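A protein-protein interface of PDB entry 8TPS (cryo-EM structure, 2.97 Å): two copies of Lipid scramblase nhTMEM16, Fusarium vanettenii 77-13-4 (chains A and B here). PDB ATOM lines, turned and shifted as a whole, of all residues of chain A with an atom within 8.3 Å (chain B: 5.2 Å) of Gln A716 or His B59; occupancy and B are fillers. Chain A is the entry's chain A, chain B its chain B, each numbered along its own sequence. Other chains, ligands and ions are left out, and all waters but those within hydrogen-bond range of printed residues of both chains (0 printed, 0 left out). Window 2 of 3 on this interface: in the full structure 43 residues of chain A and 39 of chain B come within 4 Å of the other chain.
Met A712 touches Arg B58 (CE to C, 3.6 Å). Met A712 touches Leu B65. Ile A713 touches Arg B34. Leu B65 touches Ile A713 (CD1 to CG2, 3.5 Å). Glu A714 touches Arg B34. OE1 of Gln A715 touches NE2 of His B59, 3.9 Å away. His B59 touches Gln A716.
The side-chain sulfur (SD) of Met A712 lies close to a ring nitrogen (NE2) of His B59 (3.6 Å).
Printed residues of chain B within 4 Å of Met A712: Arg B58, His B59 and Leu B65. Printed residues of chain B within 4 Å of Glu A714: Arg B34 (3.5 Å). Printed residues of chain B within 4 Å of Gln A715: His B59 (3.9 Å). Gln A716 touches one residue of chain B. Of the printed residues of chain A, Arg B34 touches Ile A713 (3.7 Å) and Glu A714 (3.5 Å). Printed residues of chain A within 4 Å of Arg B58: Met A712 (3.6 Å). Of chain A, only Met A712, Gln A715 and Gln A716 come within 4 Å of His B59. No residue of chain A comes within 4 Å of Gly B60. The nearest printed residue of chain B that does not touch Gln A716 is Arg B34 (4.9 Å).
No position is printed for both chains.
The side-chain amide nitrogen (NE2) of Gln A715 is in hydrogen-bond range of the backbone carbonyl oxygen (O) of Arg A711 (2.9 Å). The side-chain amide oxygen (OE1) of Gln A715 sits close to the side-chain sulfur (SD) of Met A712, 3.1 Å away. The backbone carbonyl oxygen (O) of Met A712 lies close to the side-chain amide oxygen (OE1) of Gln A716 (3.2 Å). The backbone NH (N) of Arg B58 sits at hydrogen-bond distance from the backbone carbonyl oxygen (O) of Leu B66 (2.9 Å). The backbone carbonyl oxygen (O) of His B59 is in hydrogen-bond range of the guanidinium group (NE) of Arg B491.
Of the 8 printed residues of chain A, 5 touch a printed residue of chain B. Hydrophobic or aromatic side chains of chain A that line the printed part of chain B: Met A712 and Ile A713. Hydrophobic or aromatic side chains of chain B within 4 Å of the printed part of chain A: His B59 and Leu B65. Along chain B the printed residues that touch a printed residue of chain A span positions 34 to 65. Among the printed residues, 8 pairs touch across the chains.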
ATOM      1  N   GLY A 709      -1.502  -6.991   4.954  1.00  0.00           N
ATOM      2  CA  GLY A 709      -0.487  -7.886   5.494  1.00  0.00           C
ATOM      3  C   GLY A 709       0.906  -7.604   4.957  1.00  0.00           C
ATOM      4  O   GLY A 709       1.891  -7.648   5.703  1.00  0.00           O
ATOM      5  N   ARG A 710       1.011  -7.325   3.655  1.00  0.00           N
ATOM      6  CA  ARG A 710       2.295  -6.943   3.078  1.00  0.00           C
ATOM      7  C   ARG A 710       2.814  -5.651   3.698  1.00  0.00           C
ATOM      8  O   ARG A 710       3.957  -5.598   4.169  1.00  0.00           O
ATOM      9  CB  ARG A 710       2.167  -6.799   1.561  1.00  0.00           C
ATOM     10  N   ARG A 711       1.984  -4.602   3.733  1.00  0.00           N
ATOM     11  CA  ARG A 711       2.425  -3.369   4.387  1.00  0.00           C
ATOM     12  C   ARG A 711       2.671  -3.590   5.876  1.00  0.00           C
ATOM     13  O   ARG A 711       3.465  -2.872   6.499  1.00  0.00           O
ATOM     14  CB  ARG A 711       1.399  -2.254   4.183  1.00  0.00           C
ATOM     15  N   MET A 712       2.023  -4.603   6.439  1.00  0.00           N
ATOM     16  CA  MET A 712       2.023  -4.879   7.862  1.00  0.00           C
ATOM     17  C   MET A 712       3.345  -5.483   8.302  1.00  0.00           C
ATOM     18  O   MET A 712       3.894  -5.106   9.343  1.00  0.00           O
ATOM     19  CB  MET A 712       0.862  -5.829   8.137  1.00  0.00           C
ATOM     20  CG  MET A 712       0.492  -6.071   9.557  1.00  0.00           C
ATOM     21  SD  MET A 712       0.853  -4.757  10.709  1.00  0.00           S
ATOM     22  CE  MET A 712       0.071  -5.508  12.118  1.00  0.00           C
ATOM     23  N   ILE A 713       3.854  -6.438   7.521  1.00  0.00           N
ATOM     24  CA  ILE A 713       5.220  -6.909   7.717  1.00  0.00           C
ATOM     25  C   ILE A 713       6.238  -5.879   7.244  1.00  0.00           C
ATOM     26  O   ILE A 713       7.369  -5.869   7.745  1.00  0.00           O
ATOM     27  CB  ILE A 713       5.475  -8.253   7.014  1.00  0.00           C
ATOM     28  CG1 ILE A 713       5.211  -8.144   5.512  1.00  0.00           C
ATOM     29  CG2 ILE A 713       4.635  -9.348   7.637  1.00  0.00           C
ATOM     30  CD1 ILE A 713       5.572  -9.396   4.736  1.00  0.00           C
ATOM     31  N   GLU A 714       5.869  -5.010   6.295  1.00  0.00           N
ATOM     32  CA  GLU A 714       6.755  -3.927   5.888  1.00  0.00           C
ATOM     33  C   GLU A 714       7.000  -2.926   7.009  1.00  0.00           C
ATOM     34  O   GLU A 714       8.062  -2.296   7.040  1.00  0.00           O
ATOM     35  CB  GLU A 714       6.179  -3.208   4.666  1.00  0.00           C
ATOM     36  N   GLN A 715       6.044  -2.762   7.929  1.00  0.00           N
ATOM     37  CA  GLN A 715       6.266  -1.862   9.056  1.00  0.00           C
ATOM     38  C   GLN A 715       7.373  -2.349   9.986  1.00  0.00           C
ATOM     39  O   GLN A 715       7.890  -1.556  10.778  1.00  0.00           O
ATOM     40  CB  GLN A 715       4.971  -1.666   9.845  1.00  0.00           C
ATOM     41  CG  GLN A 715       3.977  -0.729   9.173  1.00  0.00           C
ATOM     42  CD  GLN A 715       2.587  -1.320   9.088  1.00  0.00           C
ATOM     43  OE1 GLN A 715       2.152  -2.036   9.989  1.00  0.00           O
ATOM     44  NE2 GLN A 715       1.883  -1.032   8.000  1.00  0.00           N
ATOM     45  N   GLN A 716       7.746  -3.623   9.908  1.00  0.00           N
ATOM     46  CA  GLN A 716       8.871  -4.142  10.680  1.00  0.00           C
ATOM     47  C   GLN A 716       9.768  -5.011   9.806  1.00  0.00           C
ATOM     48  O   GLN A 716      10.953  -4.726   9.637  1.00  0.00           O
ATOM     49  CB  GLN A 716       8.384  -4.942  11.891  1.00  0.00           C
ATOM     50  CG  GLN A 716       7.303  -5.960  11.577  1.00  0.00           C
ATOM     51  CD  GLN A 716       5.930  -5.504  12.026  1.00  0.00           C
ATOM     52  OE1 GLN A 716       5.595  -4.323  11.932  1.00  0.00           O
ATOM     53  NE2 GLN A 716       5.130  -6.439  12.524  1.00  0.00           N
ATOM     54  N   ARG B  34      12.182 -14.046   4.994  1.00  0.00           N
ATOM     55  CA  ARG B  34      10.987 -13.226   4.828  1.00  0.00           C
ATOM     56  C   ARG B  34      10.357 -13.401   3.450  1.00  0.00           C
ATOM     57  O   ARG B  34       9.128 -13.317   3.308  1.00  0.00           O
ATOM     58  CB  ARG B  34      11.336 -11.758   5.072  1.00  0.00           C
ATOM     59  CG  ARG B  34      10.153 -10.813   5.044  1.00  0.00           C
ATOM     60  CD  ARG B  34      10.614  -9.398   4.753  1.00  0.00           C
ATOM     61  NE  ARG B  34       9.500  -8.509   4.451  1.00  0.00           N
ATOM     62  CZ  ARG B  34       9.520  -7.196   4.631  1.00  0.00           C
ATOM     63  NH1 ARG B  34      10.582  -6.580   5.126  1.00  0.00           N
ATOM     64  NH2 ARG B  34       8.449  -6.480   4.302  1.00  0.00           N
ATOM     65  N   VAL B  57      -6.035  -9.355  10.178  1.00  0.00           N
ATOM     66  CA  VAL B  57      -4.612  -9.427  10.511  1.00  0.00           C
ATOM     67  C   VAL B  57      -4.258  -8.281  11.447  1.00  0.00           C
ATOM     68  O   VAL B  57      -4.605  -7.126  11.178  1.00  0.00           O
ATOM     69  CB  VAL B  57      -3.720  -9.382   9.254  1.00  0.00           C
ATOM     70  CG1 VAL B  57      -2.355  -9.983   9.553  1.00  0.00           C
ATOM     71  CG2 VAL B  57      -4.382 -10.110   8.095  1.00  0.00           C
ATOM     72  N   ARG B  58      -3.554  -8.595  12.540  1.00  0.00           N
ATOM     73  CA  ARG B  58      -3.124  -7.609  13.525  1.00  0.00           C
ATOM     74  C   ARG B  58      -1.714  -7.929  14.012  1.00  0.00           C
ATOM     75  O   ARG B  58      -1.172  -9.013  13.764  1.00  0.00           O
ATOM     76  CB  ARG B  58      -4.084  -7.545  14.724  1.00  0.00           C
ATOM     77  CG  ARG B  58      -5.519  -7.190  14.380  1.00  0.00           C
ATOM     78  CD  ARG B  58      -5.613  -5.774  13.837  1.00  0.00           C
ATOM     79  NE  ARG B  58      -6.729  -5.619  12.914  1.00  0.00           N
ATOM     80  CZ  ARG B  58      -7.855  -4.979  13.203  1.00  0.00           C
ATOM     81  NH1 ARG B  58      -8.038  -4.400  14.380  1.00  0.00           N
ATOM     82  NH2 ARG B  58      -8.819  -4.916  12.290  1.00  0.00           N
ATOM     83  N   HIS B  59      -1.123  -6.963  14.721  1.00  0.00           N
ATOM     84  CA  HIS B  59       0.222  -7.132  15.261  1.00  0.00           C
ATOM     85  C   HIS B  59       0.253  -8.253  16.290  1.00  0.00           C
ATOM     86  O   HIS B  59      -0.784  -8.682  16.800  1.00  0.00           O
ATOM     87  CB  HIS B  59       0.717  -5.846  15.932  1.00  0.00           C
ATOM     88  CG  HIS B  59       1.251  -4.816  14.987  1.00  0.00           C
ATOM     89  ND1 HIS B  59       2.481  -4.934  14.376  1.00  0.00           N
ATOM     90  CD2 HIS B  59       0.754  -3.615  14.604  1.00  0.00           C
ATOM     91  CE1 HIS B  59       2.701  -3.870  13.623  1.00  0.00           C
ATOM     92  NE2 HIS B  59       1.668  -3.055  13.744  1.00  0.00           N
ATOM     93  N   GLY B  60       1.460  -8.715  16.601  1.00  0.00           N
ATOM     94  CA  GLY B  60       1.692  -9.546  17.762  1.00  0.00           C
ATOM     95  C   GLY B  60       3.099  -9.313  18.271  1.00  0.00           C
ATOM     96  O   GLY B  60       3.965  -8.826  17.541  1.00  0.00           O
ATOM     97  N   GLU B  61       3.322  -9.653  19.536  1.00  0.00           N
ATOM     98  CA  GLU B  61       4.634  -9.466  20.132  1.00  0.00           C
ATOM     99  C   GLU B  61       5.675 -10.307  19.403  1.00  0.00           C
ATOM    100  O   GLU B  61       5.412 -11.450  19.019  1.00  0.00           O
ATOM    101  CB  GLU B  61       4.605  -9.832  21.616  1.00  0.00           C
ATOM    102  N   GLU B  63       7.481  -9.897  16.293  1.00  0.00           N
ATOM    103  CA  GLU B  63       7.456 -10.098  14.836  1.00  0.00           C
ATOM    104  C   GLU B  63       6.409 -11.115  14.366  1.00  0.00           C
ATOM    105  O   GLU B  63       6.478 -11.649  13.260  1.00  0.00           O
ATOM    106  CB  GLU B  63       8.880 -10.401  14.310  1.00  0.00           C
ATOM    107  CG  GLU B  63       9.719 -11.637  14.803  1.00  0.00           C
ATOM    108  CD  GLU B  63       9.143 -13.047  14.668  1.00  0.00           C
ATOM    109  OE1 GLU B  63       9.697 -13.941  15.343  1.00  0.00           O
ATOM    110  OE2 GLU B  63       8.200 -13.308  13.907  1.00  0.00           O
ATOM    111  N   SER B  64       5.356 -11.265  15.164  1.00  0.00           N
ATOM    112  CA  SER B  64       4.294 -12.201  14.816  1.00  0.00           C
ATOM    113  C   SER B  64       3.102 -11.436  14.258  1.00  0.00           C
ATOM    114  O   SER B  64       2.864 -10.275  14.601  1.00  0.00           O
ATOM    115  CB  SER B  64       3.870 -13.043  16.024  1.00  0.00           C
ATOM    116  OG  SER B  64       3.426 -12.221  17.090  1.00  0.00           O
ATOM    117  N   LEU B  65       2.344 -12.115  13.395  1.00  0.00           N
ATOM    118  CA  LEU B  65       1.158 -11.547  12.754  1.00  0.00           C
ATOM    119  C   LEU B  65      -0.056 -12.380  13.145  1.00  0.00           C
ATOM    120  O   LEU B  65      -0.299 -13.438  12.560  1.00  0.00           O
ATOM    121  CB  LEU B  65       1.315 -11.508  11.238  1.00  0.00           C
ATOM    122  CG  LEU B  65       1.798 -10.189  10.651  1.00  0.00           C
ATOM    123  CD1 LEU B  65       1.600 -10.183   9.147  1.00  0.00           C
ATOM    124  CD2 LEU B  65       1.066  -9.037  11.306  1.00  0.00           C
ATOM    125  N   LEU B  66      -0.838 -11.898  14.110  1.00  0.00           N
ATOM    126  CA  LEU B  66      -2.001 -12.658  14.551  1.00  0.00           C
ATOM    127  C   LEU B  66      -3.113 -12.557  13.514  1.00  0.00           C
ATOM    128  O   LEU B  66      -3.440 -11.462  13.041  1.00  0.00           O
ATOM    129  CB  LEU B  66      -2.484 -12.168  15.914  1.00  0.00           C
ATOM    130  CG  LEU B  66      -1.536 -12.418  17.089  1.00  0.00           C
ATOM    131  CD1 LEU B  66      -1.680 -11.337  18.143  1.00  0.00           C
ATOM    132  CD2 LEU B  66      -1.775 -13.793  17.692  1.00  0.00           C
ATOM    133  N   ARG B 491      -2.490 -11.168  22.568  1.00  0.00           N
ATOM    134  CA  ARG B 491      -1.038 -11.315  22.543  1.00  0.00           C
ATOM    135  C   ARG B 491      -0.521 -12.003  23.800  1.00  0.00           C
ATOM    136  O   ARG B 491       0.370 -12.855  23.718  1.00  0.00           O
ATOM    137  CB  ARG B 491      -0.377  -9.946  22.376  1.00  0.00           C
ATOM    138  CG  ARG B 491      -0.453  -9.394  20.963  1.00  0.00           C
ATOM    139  CD  ARG B 491       0.323  -8.095  20.830  1.00  0.00           C
ATOM    140  NE  ARG B 491      -0.113  -7.319  19.675  1.00  0.00           N
ATOM    141  CZ  ARG B 491      -0.947  -6.290  19.735  1.00  0.00           C
ATOM    142  NH1 ARG B 491      -1.456  -5.881  20.886  1.00  0.00           N
ATOM    143  NH2 ARG B 491      -1.278  -5.655  18.615  1.00  0.00           N
